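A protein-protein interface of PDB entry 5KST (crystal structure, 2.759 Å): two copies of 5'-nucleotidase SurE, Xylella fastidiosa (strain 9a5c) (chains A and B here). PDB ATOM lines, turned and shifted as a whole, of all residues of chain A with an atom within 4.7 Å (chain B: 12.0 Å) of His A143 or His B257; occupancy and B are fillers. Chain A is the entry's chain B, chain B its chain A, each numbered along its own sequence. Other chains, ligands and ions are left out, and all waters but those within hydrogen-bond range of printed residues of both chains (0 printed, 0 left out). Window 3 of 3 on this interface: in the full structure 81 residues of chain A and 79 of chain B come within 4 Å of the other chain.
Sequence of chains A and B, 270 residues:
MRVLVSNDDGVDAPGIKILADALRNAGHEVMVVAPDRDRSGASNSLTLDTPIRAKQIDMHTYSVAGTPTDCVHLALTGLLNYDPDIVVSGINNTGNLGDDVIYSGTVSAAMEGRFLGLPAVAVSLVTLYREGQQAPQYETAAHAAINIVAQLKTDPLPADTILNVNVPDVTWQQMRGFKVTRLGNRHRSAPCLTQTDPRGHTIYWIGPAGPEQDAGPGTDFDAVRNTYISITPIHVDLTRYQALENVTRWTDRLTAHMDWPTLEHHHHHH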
ATOM      1  N   GLU A 139       5.191   9.807  17.044  1.00  0.00           N
ATOM      2  CA  GLU A 139       3.942  10.553  16.920  1.00  0.00           C
ATOM      3  C   GLU A 139       3.673  10.901  15.464  1.00  0.00           C
ATOM      4  O   GLU A 139       2.542  10.791  14.986  1.00  0.00           O
ATOM      5  CB  GLU A 139       3.978  11.827  17.763  1.00  0.00           C
ATOM      6  CG  GLU A 139       3.894  11.604  19.269  1.00  0.00           C
ATOM      7  CD  GLU A 139       5.245  11.314  19.911  1.00  0.00           C
ATOM      8  OE1 GLU A 139       5.314  11.312  21.162  1.00  0.00           O
ATOM      9  OE2 GLU A 139       6.232  11.088  19.171  1.00  0.00           O
ATOM     10  N   THR A 140       4.726  11.316  14.765  1.00  0.00           N
ATOM     11  CA  THR A 140       4.640  11.641  13.348  1.00  0.00           C
ATOM     12  C   THR A 140       4.148  10.446  12.549  1.00  0.00           C
ATOM     13  O   THR A 140       3.205  10.551  11.761  1.00  0.00           O
ATOM     14  CB  THR A 140       6.000  12.083  12.786  1.00  0.00           C
ATOM     15  OG1 THR A 140       6.516  13.176  13.560  1.00  0.00           O
ATOM     16  CG2 THR A 140       5.859  12.502  11.334  1.00  0.00           C
ATOM     17  N   ALA A 141       4.802   9.308  12.762  1.00  0.00           N
ATOM     18  CA  ALA A 141       4.417   8.064  12.126  1.00  0.00           C
ATOM     19  C   ALA A 141       3.008   7.684  12.529  1.00  0.00           C
ATOM     20  O   ALA A 141       2.221   7.236  11.702  1.00  0.00           O
ATOM     21  CB  ALA A 141       5.391   6.966  12.489  1.00  0.00           C
ATOM     22  N   ALA A 142       2.690   7.874  13.806  1.00  0.00           N
ATOM     23  CA  ALA A 142       1.351   7.592  14.319  1.00  0.00           C
ATOM     24  C   ALA A 142       0.310   8.466  13.630  1.00  0.00           C
ATOM     25  O   ALA A 142      -0.754   7.986  13.236  1.00  0.00           O
ATOM     26  CB  ALA A 142       1.302   7.795  15.822  1.00  0.00           C
ATOM     27  N   HIS A 143       0.630   9.748  13.487  1.00  0.00           N
ATOM     28  CA  HIS A 143      -0.228  10.678  12.763  1.00  0.00           C
ATOM     29  C   HIS A 143      -0.452  10.168  11.346  1.00  0.00           C
ATOM     30  O   HIS A 143      -1.578  10.165  10.846  1.00  0.00           O
ATOM     31  CB  HIS A 143       0.393  12.074  12.747  1.00  0.00           C
ATOM     32  CG  HIS A 143      -0.495  13.135  12.167  1.00  0.00           C
ATOM     33  ND1 HIS A 143      -0.291  14.478  12.406  1.00  0.00           N
ATOM     34  CD2 HIS A 143      -1.575  13.059  11.355  1.00  0.00           C
ATOM     35  CE1 HIS A 143      -1.212  15.180  11.770  1.00  0.00           C
ATOM     36  NE2 HIS A 143      -2.004  14.345  11.125  1.00  0.00           N
ATOM     37  N   ALA A 144       0.628   9.729  10.710  1.00  0.00           N
ATOM     38  CA  ALA A 144       0.546   9.147   9.376  1.00  0.00           C
ATOM     39  C   ALA A 144      -0.370   7.934   9.384  1.00  0.00           C
ATOM     40  O   ALA A 144      -1.226   7.782   8.510  1.00  0.00           O
ATOM     41  CB  ALA A 144       1.928   8.758   8.876  1.00  0.00           C
ATOM     42  N   ALA A 145      -0.186   7.083  10.391  1.00  0.00           N
ATOM     43  CA  ALA A 145      -0.945   5.850  10.518  1.00  0.00           C
ATOM     44  C   ALA A 145      -2.444   6.114  10.593  1.00  0.00           C
ATOM     45  O   ALA A 145      -3.212   5.564   9.805  1.00  0.00           O
ATOM     46  CB  ALA A 145      -0.482   5.079  11.730  1.00  0.00           C
ATOM     47  N   ILE A 146      -2.863   6.964  11.527  1.00  0.00           N
ATOM     48  CA  ILE A 146      -4.288   7.231  11.695  1.00  0.00           C
ATOM     49  C   ILE A 146      -4.866   7.906  10.449  1.00  0.00           C
ATOM     50  O   ILE A 146      -6.043   7.739  10.133  1.00  0.00           O
ATOM     51  CB  ILE A 146      -4.574   8.103  12.948  1.00  0.00           C
ATOM     52  CG1 ILE A 146      -4.178   9.561  12.711  1.00  0.00           C
ATOM     53  CG2 ILE A 146      -3.866   7.540  14.174  1.00  0.00           C
ATOM     54  CD1 ILE A 146      -4.385  10.461  13.918  1.00  0.00           C
ATOM     55  N   ASN A 147      -4.032   8.648   9.727  1.00  0.00           N
ATOM     56  CA  ASN A 147      -4.471   9.272   8.487  1.00  0.00           C
ATOM     57  C   ASN A 147      -4.687   8.231   7.403  1.00  0.00           C
ATOM     58  O   ASN A 147      -5.657   8.295   6.650  1.00  0.00           O
ATOM     59  CB  ASN A 147      -3.458  10.314   8.015  1.00  0.00           C
ATOM     60  CG  ASN A 147      -3.600  11.632   8.740  1.00  0.00           C
ATOM     61  OD1 ASN A 147      -4.233  11.710   9.793  1.00  0.00           O
ATOM     62  ND2 ASN A 147      -3.010  12.683   8.178  1.00  0.00           N
ATOM     63  N   TRP A 172       5.878  16.388  12.063  1.00  0.00           N
ATOM     64  CA  TRP A 172       4.847  16.343  11.033  1.00  0.00           C
ATOM     65  C   TRP A 172       4.869  17.595  10.165  1.00  0.00           C
ATOM     66  O   TRP A 172       4.462  17.568   9.002  1.00  0.00           O
ATOM     67  CB  TRP A 172       3.464  16.171  11.661  1.00  0.00           C
ATOM     68  CG  TRP A 172       2.365  16.030  10.648  1.00  0.00           C
ATOM     69  CD1 TRP A 172       1.536  17.019  10.189  1.00  0.00           C
ATOM     70  CD2 TRP A 172       1.980  14.834   9.961  1.00  0.00           C
ATOM     71  NE1 TRP A 172       0.658  16.507   9.263  1.00  0.00           N
ATOM     72  CE2 TRP A 172       0.911  15.169   9.104  1.00  0.00           C
ATOM     73  CE3 TRP A 172       2.434  13.513   9.988  1.00  0.00           C
ATOM     74  CZ2 TRP A 172       0.290  14.227   8.284  1.00  0.00           C
ATOM     75  CZ3 TRP A 172       1.817  12.582   9.173  1.00  0.00           C
ATOM     76  CH2 TRP A 172       0.758  12.944   8.332  1.00  0.00           C
ATOM     77  N   ARG A 176       7.107  16.669   3.943  1.00  0.00           N
ATOM     78  CA  ARG A 176       6.667  17.264   2.692  1.00  0.00           C
ATOM     79  C   ARG A 176       5.344  16.654   2.231  1.00  0.00           C
ATOM     80  O   ARG A 176       4.550  17.321   1.572  1.00  0.00           O
ATOM     81  CB  ARG A 176       7.750  17.115   1.619  1.00  0.00           C
ATOM     82  CG  ARG A 176       8.904  18.100   1.788  1.00  0.00           C
ATOM     83  CD  ARG A 176       9.971  17.931   0.716  1.00  0.00           C
ATOM     84  NE  ARG A 176      10.892  19.067   0.673  1.00  0.00           N
ATOM     85  CZ  ARG A 176      12.012  19.162   1.386  1.00  0.00           C
ATOM     86  NH1 ARG A 176      12.368  18.186   2.210  1.00  0.00           N
ATOM     87  NH2 ARG A 176      12.779  20.238   1.273  1.00  0.00           N
ATOM     88  N   GLY A 177       5.100  15.398   2.592  1.00  0.00           N
ATOM     89  CA  GLY A 177       3.848  14.755   2.231  1.00  0.00           C
ATOM     90  C   GLY A 177       3.853  13.240   2.205  1.00  0.00           C
ATOM     91  O   GLY A 177       4.723  12.597   2.791  1.00  0.00           O
ATOM     92  N   PHE A 178       2.854  12.673   1.533  1.00  0.00           N
ATOM     93  CA  PHE A 178       2.787  11.236   1.296  1.00  0.00           C
ATOM     94  C   PHE A 178       3.185  10.937  -0.139  1.00  0.00           C
ATOM     95  O   PHE A 178       2.945  11.744  -1.033  1.00  0.00           O
ATOM     96  CB  PHE A 178       1.383  10.694   1.555  1.00  0.00           C
ATOM     97  CG  PHE A 178       0.957  10.740   2.988  1.00  0.00           C
ATOM     98  CD1 PHE A 178       0.481  11.916   3.545  1.00  0.00           C
ATOM     99  CD2 PHE A 178       0.991   9.596   3.768  1.00  0.00           C
ATOM    100  CE1 PHE A 178       0.068  11.955   4.864  1.00  0.00           C
ATOM    101  CE2 PHE A 178       0.576   9.627   5.087  1.00  0.00           C
ATOM    102  CZ  PHE A 178       0.116  10.806   5.636  1.00  0.00           C
ATOM    103  N   THR B 248      -2.347   5.664  -5.059  1.00  0.00           N
ATOM    104  CA  THR B 248      -1.947   7.023  -5.394  1.00  0.00           C
ATOM    105  C   THR B 248      -3.131   7.973  -5.317  1.00  0.00           C
ATOM    106  O   THR B 248      -2.983   9.134  -4.934  1.00  0.00           O
ATOM    107  CB  THR B 248      -1.326   7.088  -6.798  1.00  0.00           C
ATOM    108  OG1 THR B 248      -0.225   6.174  -6.870  1.00  0.00           O
ATOM    109  CG2 THR B 248      -0.835   8.495  -7.107  1.00  0.00           C
ATOM    110  N   TRP B 250      -5.862   8.082  -3.308  1.00  0.00           N
ATOM    111  CA  TRP B 250      -6.222   8.621  -1.997  1.00  0.00           C
ATOM    112  C   TRP B 250      -4.996   9.087  -1.216  1.00  0.00           C
ATOM    113  O   TRP B 250      -5.117   9.708  -0.158  1.00  0.00           O
ATOM    114  CB  TRP B 250      -7.020   7.601  -1.176  1.00  0.00           C
ATOM    115  CG  TRP B 250      -6.338   6.299  -0.921  1.00  0.00           C
ATOM    116  CD1 TRP B 250      -6.520   5.135  -1.605  1.00  0.00           C
ATOM    117  CD2 TRP B 250      -5.387   6.015   0.108  1.00  0.00           C
ATOM    118  NE1 TRP B 250      -5.734   4.147  -1.071  1.00  0.00           N
ATOM    119  CE2 TRP B 250      -5.027   4.664  -0.019  1.00  0.00           C
ATOM    120  CE3 TRP B 250      -4.797   6.776   1.119  1.00  0.00           C
ATOM    121  CZ2 TRP B 250      -4.108   4.056   0.825  1.00  0.00           C
ATOM    122  CZ3 TRP B 250      -3.884   6.171   1.957  1.00  0.00           C
ATOM    123  CH2 TRP B 250      -3.547   4.825   1.805  1.00  0.00           C
ATOM    124  N   THR B 251      -3.816   8.796  -1.751  1.00  0.00           N
ATOM    125  CA  THR B 251      -2.578   9.273  -1.156  1.00  0.00           C
ATOM    126  C   THR B 251      -2.397  10.766  -1.449  1.00  0.00           C
ATOM    127  O   THR B 251      -1.931  11.529  -0.598  1.00  0.00           O
ATOM    128  CB  THR B 251      -1.372   8.473  -1.678  1.00  0.00           C
ATOM    129  OG1 THR B 251      -1.523   7.099  -1.306  1.00  0.00           O
ATOM    130  CG2 THR B 251      -0.071   9.000  -1.106  1.00  0.00           C
ATOM    131  N   ASP B 252      -2.781  11.175  -2.656  1.00  0.00           N
ATOM    132  CA  ASP B 252      -2.687  12.572  -3.054  1.00  0.00           C
ATOM    133  C   ASP B 252      -3.542  13.450  -2.149  1.00  0.00           C
ATOM    134  O   ASP B 252      -3.183  14.589  -1.852  1.00  0.00           O
ATOM    135  CB  ASP B 252      -3.110  12.744  -4.514  1.00  0.00           C
ATOM    136  CG  ASP B 252      -2.112  12.147  -5.490  1.00  0.00           C
ATOM    137  OD1 ASP B 252      -0.919  12.011  -5.132  1.00  0.00           O
ATOM    138  OD2 ASP B 252      -2.519  11.824  -6.626  1.00  0.00           O
ATOM    139  N   ARG B 253      -4.674  12.907  -1.711  1.00  0.00           N
ATOM    140  CA  ARG B 253      -5.564  13.608  -0.789  1.00  0.00           C
ATOM    141  C   ARG B 253      -4.854  13.900   0.524  1.00  0.00           C
ATOM    142  O   ARG B 253      -4.966  14.989   1.082  1.00  0.00           O
ATOM    143  CB  ARG B 253      -6.826  12.778  -0.502  1.00  0.00           C
ATOM    144  CG  ARG B 253      -7.524  12.212  -1.726  1.00  0.00           C
ATOM    145  CD  ARG B 253      -8.758  11.404  -1.338  1.00  0.00           C
ATOM    146  N   LEU B 254      -4.116  12.905   1.006  1.00  0.00           N
ATOM    147  CA  LEU B 254      -3.456  12.988   2.303  1.00  0.00           C
ATOM    148  C   LEU B 254      -2.397  14.091   2.357  1.00  0.00           C
ATOM    149  O   LEU B 254      -1.853  14.389   3.421  1.00  0.00           O
ATOM    150  CB  LEU B 254      -2.842  11.634   2.660  1.00  0.00           C
ATOM    151  CG  LEU B 254      -3.843  10.563   3.096  1.00  0.00           C
ATOM    152  CD1 LEU B 254      -3.142   9.254   3.391  1.00  0.00           C
ATOM    153  CD2 LEU B 254      -4.615  11.041   4.313  1.00  0.00           C
ATOM    154  N   THR B 255      -2.138  14.724   1.218  1.00  0.00           N
ATOM    155  CA  THR B 255      -1.290  15.908   1.179  1.00  0.00           C
ATOM    156  C   THR B 255      -2.051  17.102   1.785  1.00  0.00           C
ATOM    157  O   THR B 255      -1.485  18.175   2.010  1.00  0.00           O
ATOM    158  CB  THR B 255      -0.822  16.207  -0.262  1.00  0.00           C
ATOM    159  OG1 THR B 255      -0.295  15.006  -0.843  1.00  0.00           O
ATOM    160  CG2 THR B 255       0.266  17.279  -0.279  1.00  0.00           C
ATOM    161  N   ALA B 256      -3.342  16.904   2.052  1.00  0.00           N
ATOM    162  CA  ALA B 256      -4.079  17.773   2.967  1.00  0.00           C
ATOM    163  C   ALA B 256      -3.779  17.313   4.394  1.00  0.00           C
ATOM    164  O   ALA B 256      -4.550  16.555   4.986  1.00  0.00           O
ATOM    165  CB  ALA B 256      -5.570  17.731   2.682  1.00  0.00           C
ATOM    166  N   HIS B 257      -2.653  17.778   4.933  1.00  0.00           N
ATOM    167  CA  HIS B 257      -2.059  17.211   6.146  1.00  0.00           C
ATOM    168  C   HIS B 257      -2.663  17.689   7.458  1.00  0.00           C
ATOM    169  O   HIS B 257      -2.591  16.974   8.461  1.00  0.00           O
ATOM    170  CB  HIS B 257      -0.556  17.492   6.170  1.00  0.00           C
ATOM    171  CG  HIS B 257       0.212  16.727   5.141  1.00  0.00           C
ATOM    172  ND1 HIS B 257       0.578  15.407   5.313  1.00  0.00           N
ATOM    173  CD2 HIS B 257       0.679  17.090   3.924  1.00  0.00           C
ATOM    174  CE1 HIS B 257       1.237  14.994   4.248  1.00  0.00           C
ATOM    175  NE2 HIS B 257       1.310  15.994   3.388  1.00  0.00           N
ATOM    176  N   MET B 258      -3.238  18.890   7.462  1.00  0.00           N
ATOM    177  CA  MET B 258      -3.877  19.415   8.665  1.00  0.00           C
ATOM    178  C   MET B 258      -5.053  18.524   9.078  1.00  0.00           C
ATOM    179  O   MET B 258      -6.184  18.715   8.620  1.00  0.00           O
ATOM    180  CB  MET B 258      -4.338  20.858   8.450  1.00  0.00           C
ATOM    181  N   ASP B 259      -4.757  17.554   9.946  1.00  0.00           N
ATOM    182  CA  ASP B 259      -5.708  16.524  10.367  1.00  0.00           C
ATOM    183  C   ASP B 259      -6.247  15.758   9.165  1.00  0.00           C
ATOM    184  O   ASP B 259      -5.484  15.125   8.436  1.00  0.00           O
ATOM    185  CB  ASP B 259      -6.858  17.135  11.178  1.00  0.00           C
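No position is printed for both chains.
The backbone carbonyl oxygen of His B257 lies within hydrogen-bond range of the indole nitrogen of Trp A172 (3.4 Å).
The backbone carbonyl oxygen (O) of Asp B259 lies within hydrogen-bond range of the side-chain amide nitrogen (ND2) of Asn A147, 3.5 Å away.
NE2 of His A143 touches O of His B257 (3.8 Å).
Asn A147 touches Leu B254.
Arg A176 touches His B257 (O to NE2, 3.9 Å).
Gly A177 touches His B257.
CB of Phe A178 touches CG2 of Thr B251, at 3.5 Å.
Leu B254 touches Phe A178.
His B257 touches Phe A178 (CE1 to CD1, 3.2 Å).
Hydrophobic or aromatic side chains of chain A within 4 Å of the printed part of chain B: His A143, Trp A172 and Phe A178.
Printed residues of chain B that touch a printed residue of chain A: Thr B251, Leu B254, His B257 and Asp B259.
Hydrophobic or aromatic side chains of chain B that line the printed part of chain A: Leu B254 and His B257.
Along chain B the printed residues that touch a printed residue of chain A span positions 251 to 259.
Among the printed residues, no Asp or Glu carboxylate lies within 4 Å of a Lys or Arg side-chain nitrogen of the other chain.
Of chain B, only His B257 (3.8 Å) comes within 4 Å of His A143.
Printed residues of chain A within 4 Å of His B257: His A143 (3.8 Å), Trp A172 (3.2 Å), Arg A176 (3.9 Å), Gly A177 (3.1 Å) and Phe A178 (3.2 Å).
No residue of chain B comes within 4 Å of Ala A141.
No residue of chain B comes within 4 Å of Ala A142.
No residue of chain B comes within 4 Å of Ala A144.
No residue of chain B comes within 4 Å of Ile A146.
Asn A147 touches just these residues of chain B: Leu B254 and Asp B259.
Of chain B, only His B257 (3.1 Å) comes within 4 Å of Gly A177.
Of chain B, only Thr B251, Leu B254 and His B257 come within 4 Å of Phe A178.
Of the printed residues of chain A, Thr B251 touches Phe A178 (3.5 Å).
Of the printed residues of chain A, Leu B254 touches Asn A147 and Phe A178.
Of the printed residues of chain B, Arg A176 touches His B257 (3.9 Å).
Of the printed residues of chain A, Asp B259 touches Asn A147 (3.5 Å).
A ring nitrogen (ND1) of His B257 lies within hydrogen-bond range of the backbone carbonyl oxygen of Leu B254, at 3.2 Å.
The side-chain amide oxygen of Asn A147 lies close to the backbone carbonyl oxygen of His A143 (3.2 Å).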
